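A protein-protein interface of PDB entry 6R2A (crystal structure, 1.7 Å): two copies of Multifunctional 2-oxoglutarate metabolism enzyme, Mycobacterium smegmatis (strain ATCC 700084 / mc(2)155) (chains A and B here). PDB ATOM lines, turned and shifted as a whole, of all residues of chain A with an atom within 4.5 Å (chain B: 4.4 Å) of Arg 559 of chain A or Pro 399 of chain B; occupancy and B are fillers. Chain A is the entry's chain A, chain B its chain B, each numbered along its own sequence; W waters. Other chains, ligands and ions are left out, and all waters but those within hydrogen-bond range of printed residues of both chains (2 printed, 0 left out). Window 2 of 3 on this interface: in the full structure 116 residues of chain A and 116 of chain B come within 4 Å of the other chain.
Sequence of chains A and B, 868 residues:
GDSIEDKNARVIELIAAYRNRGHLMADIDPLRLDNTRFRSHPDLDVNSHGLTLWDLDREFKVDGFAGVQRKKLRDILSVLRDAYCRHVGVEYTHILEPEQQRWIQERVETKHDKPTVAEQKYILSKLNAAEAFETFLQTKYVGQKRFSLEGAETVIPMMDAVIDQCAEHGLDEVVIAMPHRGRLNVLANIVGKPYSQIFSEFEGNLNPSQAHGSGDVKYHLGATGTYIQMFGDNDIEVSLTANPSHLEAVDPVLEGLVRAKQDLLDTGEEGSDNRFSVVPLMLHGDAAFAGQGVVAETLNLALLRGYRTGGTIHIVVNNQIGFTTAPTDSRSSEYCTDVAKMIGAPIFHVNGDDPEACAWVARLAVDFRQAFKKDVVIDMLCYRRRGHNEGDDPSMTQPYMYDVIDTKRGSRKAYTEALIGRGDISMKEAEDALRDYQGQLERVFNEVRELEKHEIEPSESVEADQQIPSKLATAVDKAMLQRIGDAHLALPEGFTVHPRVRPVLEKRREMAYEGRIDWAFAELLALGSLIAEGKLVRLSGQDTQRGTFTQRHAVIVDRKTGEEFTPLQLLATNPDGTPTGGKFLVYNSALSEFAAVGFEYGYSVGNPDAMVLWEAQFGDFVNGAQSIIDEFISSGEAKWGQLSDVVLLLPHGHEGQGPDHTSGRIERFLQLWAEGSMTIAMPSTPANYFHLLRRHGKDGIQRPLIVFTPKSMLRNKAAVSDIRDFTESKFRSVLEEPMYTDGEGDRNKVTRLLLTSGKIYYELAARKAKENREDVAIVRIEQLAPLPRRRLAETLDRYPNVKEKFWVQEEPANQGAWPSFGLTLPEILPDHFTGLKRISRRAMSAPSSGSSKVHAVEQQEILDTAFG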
ATOM      1  N   THR A 496      23.291  10.531   0.212  1.00  0.00           N
ATOM      2  CA  THR A 496      22.518  11.346  -0.722  1.00  0.00           C
ATOM      3  C   THR A 496      22.091  10.468  -1.900  1.00  0.00           C
ATOM      4  O   THR A 496      22.929  10.096  -2.716  1.00  0.00           O
ATOM      5  CB  THR A 496      23.329  12.571  -1.191  1.00  0.00           C
ATOM      6  OG1 THR A 496      23.842  13.266  -0.054  1.00  0.00           O
ATOM      7  CG2 THR A 496      22.505  13.517  -2.057  1.00  0.00           C
ATOM      8  N   VAL A 497      20.797  10.151  -1.992  1.00  0.00           N
ATOM      9  CA  VAL A 497      20.279   9.347  -3.102  1.00  0.00           C
ATOM     10  C   VAL A 497      20.101  10.238  -4.322  1.00  0.00           C
ATOM     11  O   VAL A 497      19.671  11.390  -4.186  1.00  0.00           O
ATOM     12  CB  VAL A 497      18.949   8.628  -2.744  1.00  0.00           C
ATOM     13  CG1 VAL A 497      18.488   7.702  -3.884  1.00  0.00           C
ATOM     14  CG2 VAL A 497      19.093   7.840  -1.450  1.00  0.00           C
ATOM     15  N   HIS A 498      20.429   9.705  -5.517  1.00  0.00           N
ATOM     16  CA  HIS A 498      20.207  10.419  -6.773  1.00  0.00           C
ATOM     17  C   HIS A 498      18.713  10.727  -6.868  1.00  0.00           C
ATOM     18  O   HIS A 498      17.907   9.847  -6.544  1.00  0.00           O
ATOM     19  CB  HIS A 498      20.674   9.562  -7.957  1.00  0.00           C
ATOM     20  CG  HIS A 498      20.628  10.266  -9.279  1.00  0.00           C
ATOM     21  ND1 HIS A 498      19.432  10.466  -9.956  1.00  0.00           N
ATOM     22  CD2 HIS A 498      21.644  10.744 -10.034  1.00  0.00           C
ATOM     23  CE1 HIS A 498      19.756  11.075 -11.085  1.00  0.00           C
ATOM     24  NE2 HIS A 498      21.077  11.251 -11.184  1.00  0.00           N
ATOM     25  N   VAL A 557      24.317   4.665  -5.808  1.00  0.00           N
ATOM     26  CA  VAL A 557      25.535   5.455  -5.685  1.00  0.00           C
ATOM     27  C   VAL A 557      25.209   6.822  -5.108  1.00  0.00           C
ATOM     28  O   VAL A 557      24.313   7.513  -5.605  1.00  0.00           O
ATOM     29  CB  VAL A 557      26.237   5.563  -7.073  1.00  0.00           C
ATOM     30  CG1 VAL A 557      27.515   6.398  -6.990  1.00  0.00           C
ATOM     31  CG2 VAL A 557      26.526   4.183  -7.663  1.00  0.00           C
ATOM     32  N   ASP A 558      25.940   7.209  -4.057  1.00  0.00           N
ATOM     33  CA  ASP A 558      25.764   8.492  -3.385  1.00  0.00           C
ATOM     34  C   ASP A 558      26.077   9.612  -4.381  1.00  0.00           C
ATOM     35  O   ASP A 558      27.174   9.642  -4.943  1.00  0.00           O
ATOM     36  CB  ASP A 558      26.664   8.565  -2.140  1.00  0.00           C
ATOM     37  CG  ASP A 558      26.440   9.807  -1.300  1.00  0.00           C
ATOM     38  OD1 ASP A 558      26.618  10.930  -1.833  1.00  0.00           O
ATOM     39  OD2 ASP A 558      26.098   9.660  -0.112  1.00  0.00           O
ATOM     40  N   ARG A 559      25.093  10.499  -4.626  1.00  0.00           N
ATOM     41  CA  ARG A 559      25.163  11.582  -5.612  1.00  0.00           C
ATOM     42  C   ARG A 559      26.307  12.565  -5.335  1.00  0.00           C
ATOM     43  O   ARG A 559      26.822  13.170  -6.280  1.00  0.00           O
ATOM     44  CB  ARG A 559      23.811  12.334  -5.684  1.00  0.00           C
ATOM     45  CG  ARG A 559      23.690  13.470  -6.726  1.00  0.00           C
ATOM     46  CD  ARG A 559      23.891  12.995  -8.166  1.00  0.00           C
ATOM     47  NE  ARG A 559      23.937  14.103  -9.126  1.00  0.00           N
ATOM     48  CZ  ARG A 559      25.025  14.820  -9.401  1.00  0.00           C
ATOM     49  NH1 ARG A 559      26.170  14.569  -8.779  1.00  0.00           N
ATOM     50  NH2 ARG A 559      24.969  15.804 -10.288  1.00  0.00           N
ATOM     51  N   LYS A 560      26.712  12.703  -4.065  1.00  0.00           N
ATOM     52  CA  LYS A 560      27.738  13.660  -3.662  1.00  0.00           C
ATOM     53  C   LYS A 560      29.119  13.042  -3.475  1.00  0.00           C
ATOM     54  O   LYS A 560      30.112  13.738  -3.704  1.00  0.00           O
ATOM     55  CB  LYS A 560      27.318  14.378  -2.356  1.00  0.00           C
ATOM     56  CG  LYS A 560      26.189  15.385  -2.560  1.00  0.00           C
ATOM     57  CD  LYS A 560      25.579  15.840  -1.239  1.00  0.00           C
ATOM     58  CE  LYS A 560      25.898  17.272  -0.903  1.00  0.00           C
ATOM     59  NZ  LYS A 560      25.176  17.707   0.321  1.00  0.00           N
ATOM     60  N   THR A 561      29.206  11.770  -3.036  1.00  0.00           N
ATOM     61  CA  THR A 561      30.498  11.152  -2.714  1.00  0.00           C
ATOM     62  C   THR A 561      30.880   9.930  -3.558  1.00  0.00           C
ATOM     63  O   THR A 561      32.028   9.484  -3.481  1.00  0.00           O
ATOM     64  CB  THR A 561      30.509  10.705  -1.236  1.00  0.00           C
ATOM     65  OG1 THR A 561      29.621   9.596  -1.080  1.00  0.00           O
ATOM     66  CG2 THR A 561      30.153  11.826  -0.261  1.00  0.00           C
ATOM     67  N   SER B 395      24.349  10.062 -14.616  1.00  0.00           N
ATOM     68  CA  SER B 395      24.709  10.570 -13.288  1.00  0.00           C
ATOM     69  C   SER B 395      24.243   9.630 -12.155  1.00  0.00           C
ATOM     70  O   SER B 395      24.767   9.715 -11.046  1.00  0.00           O
ATOM     71  CB  SER B 395      24.154  11.984 -13.064  1.00  0.00           C
ATOM     72  OG  SER B 395      22.751  12.036 -13.260  1.00  0.00           O
ATOM     73  N   THR B 397      24.867   6.419 -11.890  1.00  0.00           N
ATOM     74  CA  THR B 397      25.983   5.510 -11.601  1.00  0.00           C
ATOM     75  C   THR B 397      27.356   6.183 -11.650  1.00  0.00           C
ATOM     76  O   THR B 397      28.280   5.683 -11.005  1.00  0.00           O
ATOM     77  CB  THR B 397      25.937   4.300 -12.560  1.00  0.00           C
ATOM     78  OG1 THR B 397      25.856   4.766 -13.917  1.00  0.00           O
ATOM     79  CG2 THR B 397      24.749   3.384 -12.262  1.00  0.00           C
ATOM     80  N   GLN B 398      27.505   7.291 -12.404  1.00  0.00           N
ATOM     81  CA  GLN B 398      28.783   8.014 -12.526  1.00  0.00           C
ATOM     82  C   GLN B 398      28.566   9.494 -12.180  1.00  0.00           C
ATOM     83  O   GLN B 398      28.747  10.345 -13.050  1.00  0.00           O
ATOM     84  CB  GLN B 398      29.365   7.867 -13.943  1.00  0.00           C
ATOM     85  CG  GLN B 398      30.199   6.611 -14.127  1.00  0.00           C
ATOM     86  CD  GLN B 398      29.373   5.372 -14.277  1.00  0.00           C
ATOM     87  OE1 GLN B 398      28.293   5.374 -14.908  1.00  0.00           O
ATOM     88  NE2 GLN B 398      29.875   4.285 -13.689  1.00  0.00           N
ATOM     89  N   PRO B 399      28.137   9.823 -10.931  1.00  0.00           N
ATOM     90  CA  PRO B 399      27.826  11.232 -10.621  1.00  0.00           C
ATOM     91  C   PRO B 399      29.045  12.146 -10.713  1.00  0.00           C
ATOM     92  O   PRO B 399      28.907  13.263 -11.215  1.00  0.00           O
ATOM     93  CB  PRO B 399      27.268  11.177  -9.185  1.00  0.00           C
ATOM     94  CG  PRO B 399      27.837   9.899  -8.604  1.00  0.00           C
ATOM     95  CD  PRO B 399      27.847   8.946  -9.776  1.00  0.00           C
ATOM     96  N   TYR B 400      30.221  11.673 -10.264  1.00  0.00           N
ATOM     97  CA  TYR B 400      31.445  12.481 -10.277  1.00  0.00           C
ATOM     98  C   TYR B 400      31.911  12.768 -11.700  1.00  0.00           C
ATOM     99  O   TYR B 400      32.173  13.924 -12.033  1.00  0.00           O
ATOM    100  CB  TYR B 400      32.575  11.827  -9.473  1.00  0.00           C
ATOM    101  CG  TYR B 400      33.853  12.644  -9.481  1.00  0.00           C
ATOM    102  CD1 TYR B 400      33.888  13.928  -8.944  1.00  0.00           C
ATOM    103  CD2 TYR B 400      35.025  12.129 -10.017  1.00  0.00           C
ATOM    104  CE1 TYR B 400      35.053  14.695  -8.974  1.00  0.00           C
ATOM    105  CE2 TYR B 400      36.202  12.880 -10.035  1.00  0.00           C
ATOM    106  CZ  TYR B 400      36.210  14.163  -9.515  1.00  0.00           C
ATOM    107  OH  TYR B 400      37.364  14.907  -9.530  1.00  0.00           O
ATOM    108  N   MET B 401      31.975  11.729 -12.538  1.00  0.00           N
ATOM    109  CA  MET B 401      32.379  11.898 -13.931  1.00  0.00           C
ATOM    110  C   MET B 401      31.489  12.927 -14.635  1.00  0.00           C
ATOM    111  O   MET B 401      32.009  13.786 -15.347  1.00  0.00           O
ATOM    112  CB  MET B 401      32.322  10.537 -14.669  1.00  0.00           C
ATOM    113  CG  MET B 401      32.518  10.663 -16.173  1.00  0.00           C
ATOM    114  SD  MET B 401      32.393   9.099 -17.078  1.00  0.00           S
ATOM    115  CE  MET B 401      33.974   8.478 -16.784  1.00  0.00           C
ATOM    116  N   TYR B 402      30.165  12.863 -14.427  1.00  0.00           N
ATOM    117  CA  TYR B 402      29.260  13.755 -15.146  1.00  0.00           C
ATOM    118  C   TYR B 402      29.245  15.152 -14.528  1.00  0.00           C
ATOM    119  O   TYR B 402      29.038  16.111 -15.275  1.00  0.00           O
ATOM    120  CB  TYR B 402      27.870  13.132 -15.333  1.00  0.00           C
ATOM    121  CG  TYR B 402      27.999  12.205 -16.522  1.00  0.00           C
ATOM    122  CD1 TYR B 402      27.841  12.690 -17.822  1.00  0.00           C
ATOM    123  CD2 TYR B 402      28.517  10.915 -16.369  1.00  0.00           C
ATOM    124  CE1 TYR B 402      28.141  11.904 -18.934  1.00  0.00           C
ATOM    125  CE2 TYR B 402      28.848  10.129 -17.475  1.00  0.00           C
ATOM    126  CZ  TYR B 402      28.634  10.620 -18.755  1.00  0.00           C
ATOM    127  OH  TYR B 402      28.942   9.851 -19.843  1.00  0.00           O
ATOM    128  N   ASP B 403      29.635  15.298 -13.248  1.00  0.00           N
ATOM    129  CA  ASP B 403      29.803  16.642 -12.692  1.00  0.00           C
ATOM    130  C   ASP B 403      31.012  17.318 -13.369  1.00  0.00           C
ATOM    131  O   ASP B 403      30.928  18.497 -13.701  1.00  0.00           O
ATOM    132  CB  ASP B 403      29.955  16.599 -11.168  1.00  0.00           C
ATOM    133  CG  ASP B 403      28.632  16.431 -10.439  1.00  0.00           C
ATOM    134  OD1 ASP B 403      27.571  16.673 -11.062  1.00  0.00           O
ATOM    135  OD2 ASP B 403      28.656  16.069  -9.251  1.00  0.00           O
HETATM  136  O   HOH W   1      26.545  14.432 -12.215  1.00  0.00           O
HETATM  137  O   HOH W   2      24.233   9.258  -7.886  1.00  0.00           O
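OG of Ser 395 of chain B lies within hydrogen-bond range of NE2 of His 498 of chain A (2.8 Å). The guanidinium group of Arg 559 of chain A is in salt-bridge range of the side-chain carboxylate of Asp 403 of chain B, 2.9 Å away.
N of Thr 496 of chain A is in hydrogen-bond range of OD2 of Asp 558 of chain A, at 3.0 Å. The backbone NH of Arg 559 of chain A is in hydrogen-bond range of the backbone carbonyl oxygen of Thr 496 of chain A (2.9 Å). The side-chain carboxylate of Asp 558 of chain A is in hydrogen-bond range of the backbone NH of Lys 560 of chain A (2.9 Å). OD1 of Asp 558 of chain A is in hydrogen-bond range of N of Thr 561 of chain A (3.0 Å).
Pro 399 of chain B touches Val 557 of chain A. Pro 399 of chain B touches Asp 558 of chain A. Pro 399 of chain B touches Arg 559 of chain A.
Of chain B, only Pro 399 (3.6 Å) and Asp 403 (2.9 Å) come within 4 Å of Arg 559 of chain A. Of the printed residues of chain A, Ser 395 of chain B touches His 498 (2.8 Å). Printed residues of chain A within 4 Å of Pro 399 of chain B: Val 557, Asp 558 and Arg 559. Met 401 of chain B touches none of the printed residues of chain A. Of the printed residues of chain A, Asp 403 of chain B touches Arg 559 (2.9 Å).
Printed residues of chain B that touch a printed residue of chain A: Ser 395, Pro 399 and Asp 403. Hydrophobic or aromatic side chains of chain B that line the printed part of chain A: Pro 399. Among the printed residues, 5 pairs touch across the chains.
No position is printed for both chains. Of the 5 pairs that touch across the chains among the printed residues, none has its exchanged pair printed and touching as well.
Water W1 lies within hydrogen-bond range of the side-chain carboxylate of Asp 403 of chain B, the backbone carbonyl oxygen of Pro 399 of chain B and the guanidinium group of Arg 559 of chain A. Water W2 lies within hydrogen-bond range of O of Val 557 of chain A (2.9 Å) and O of Ser 395 of chain B (3.2 Å).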
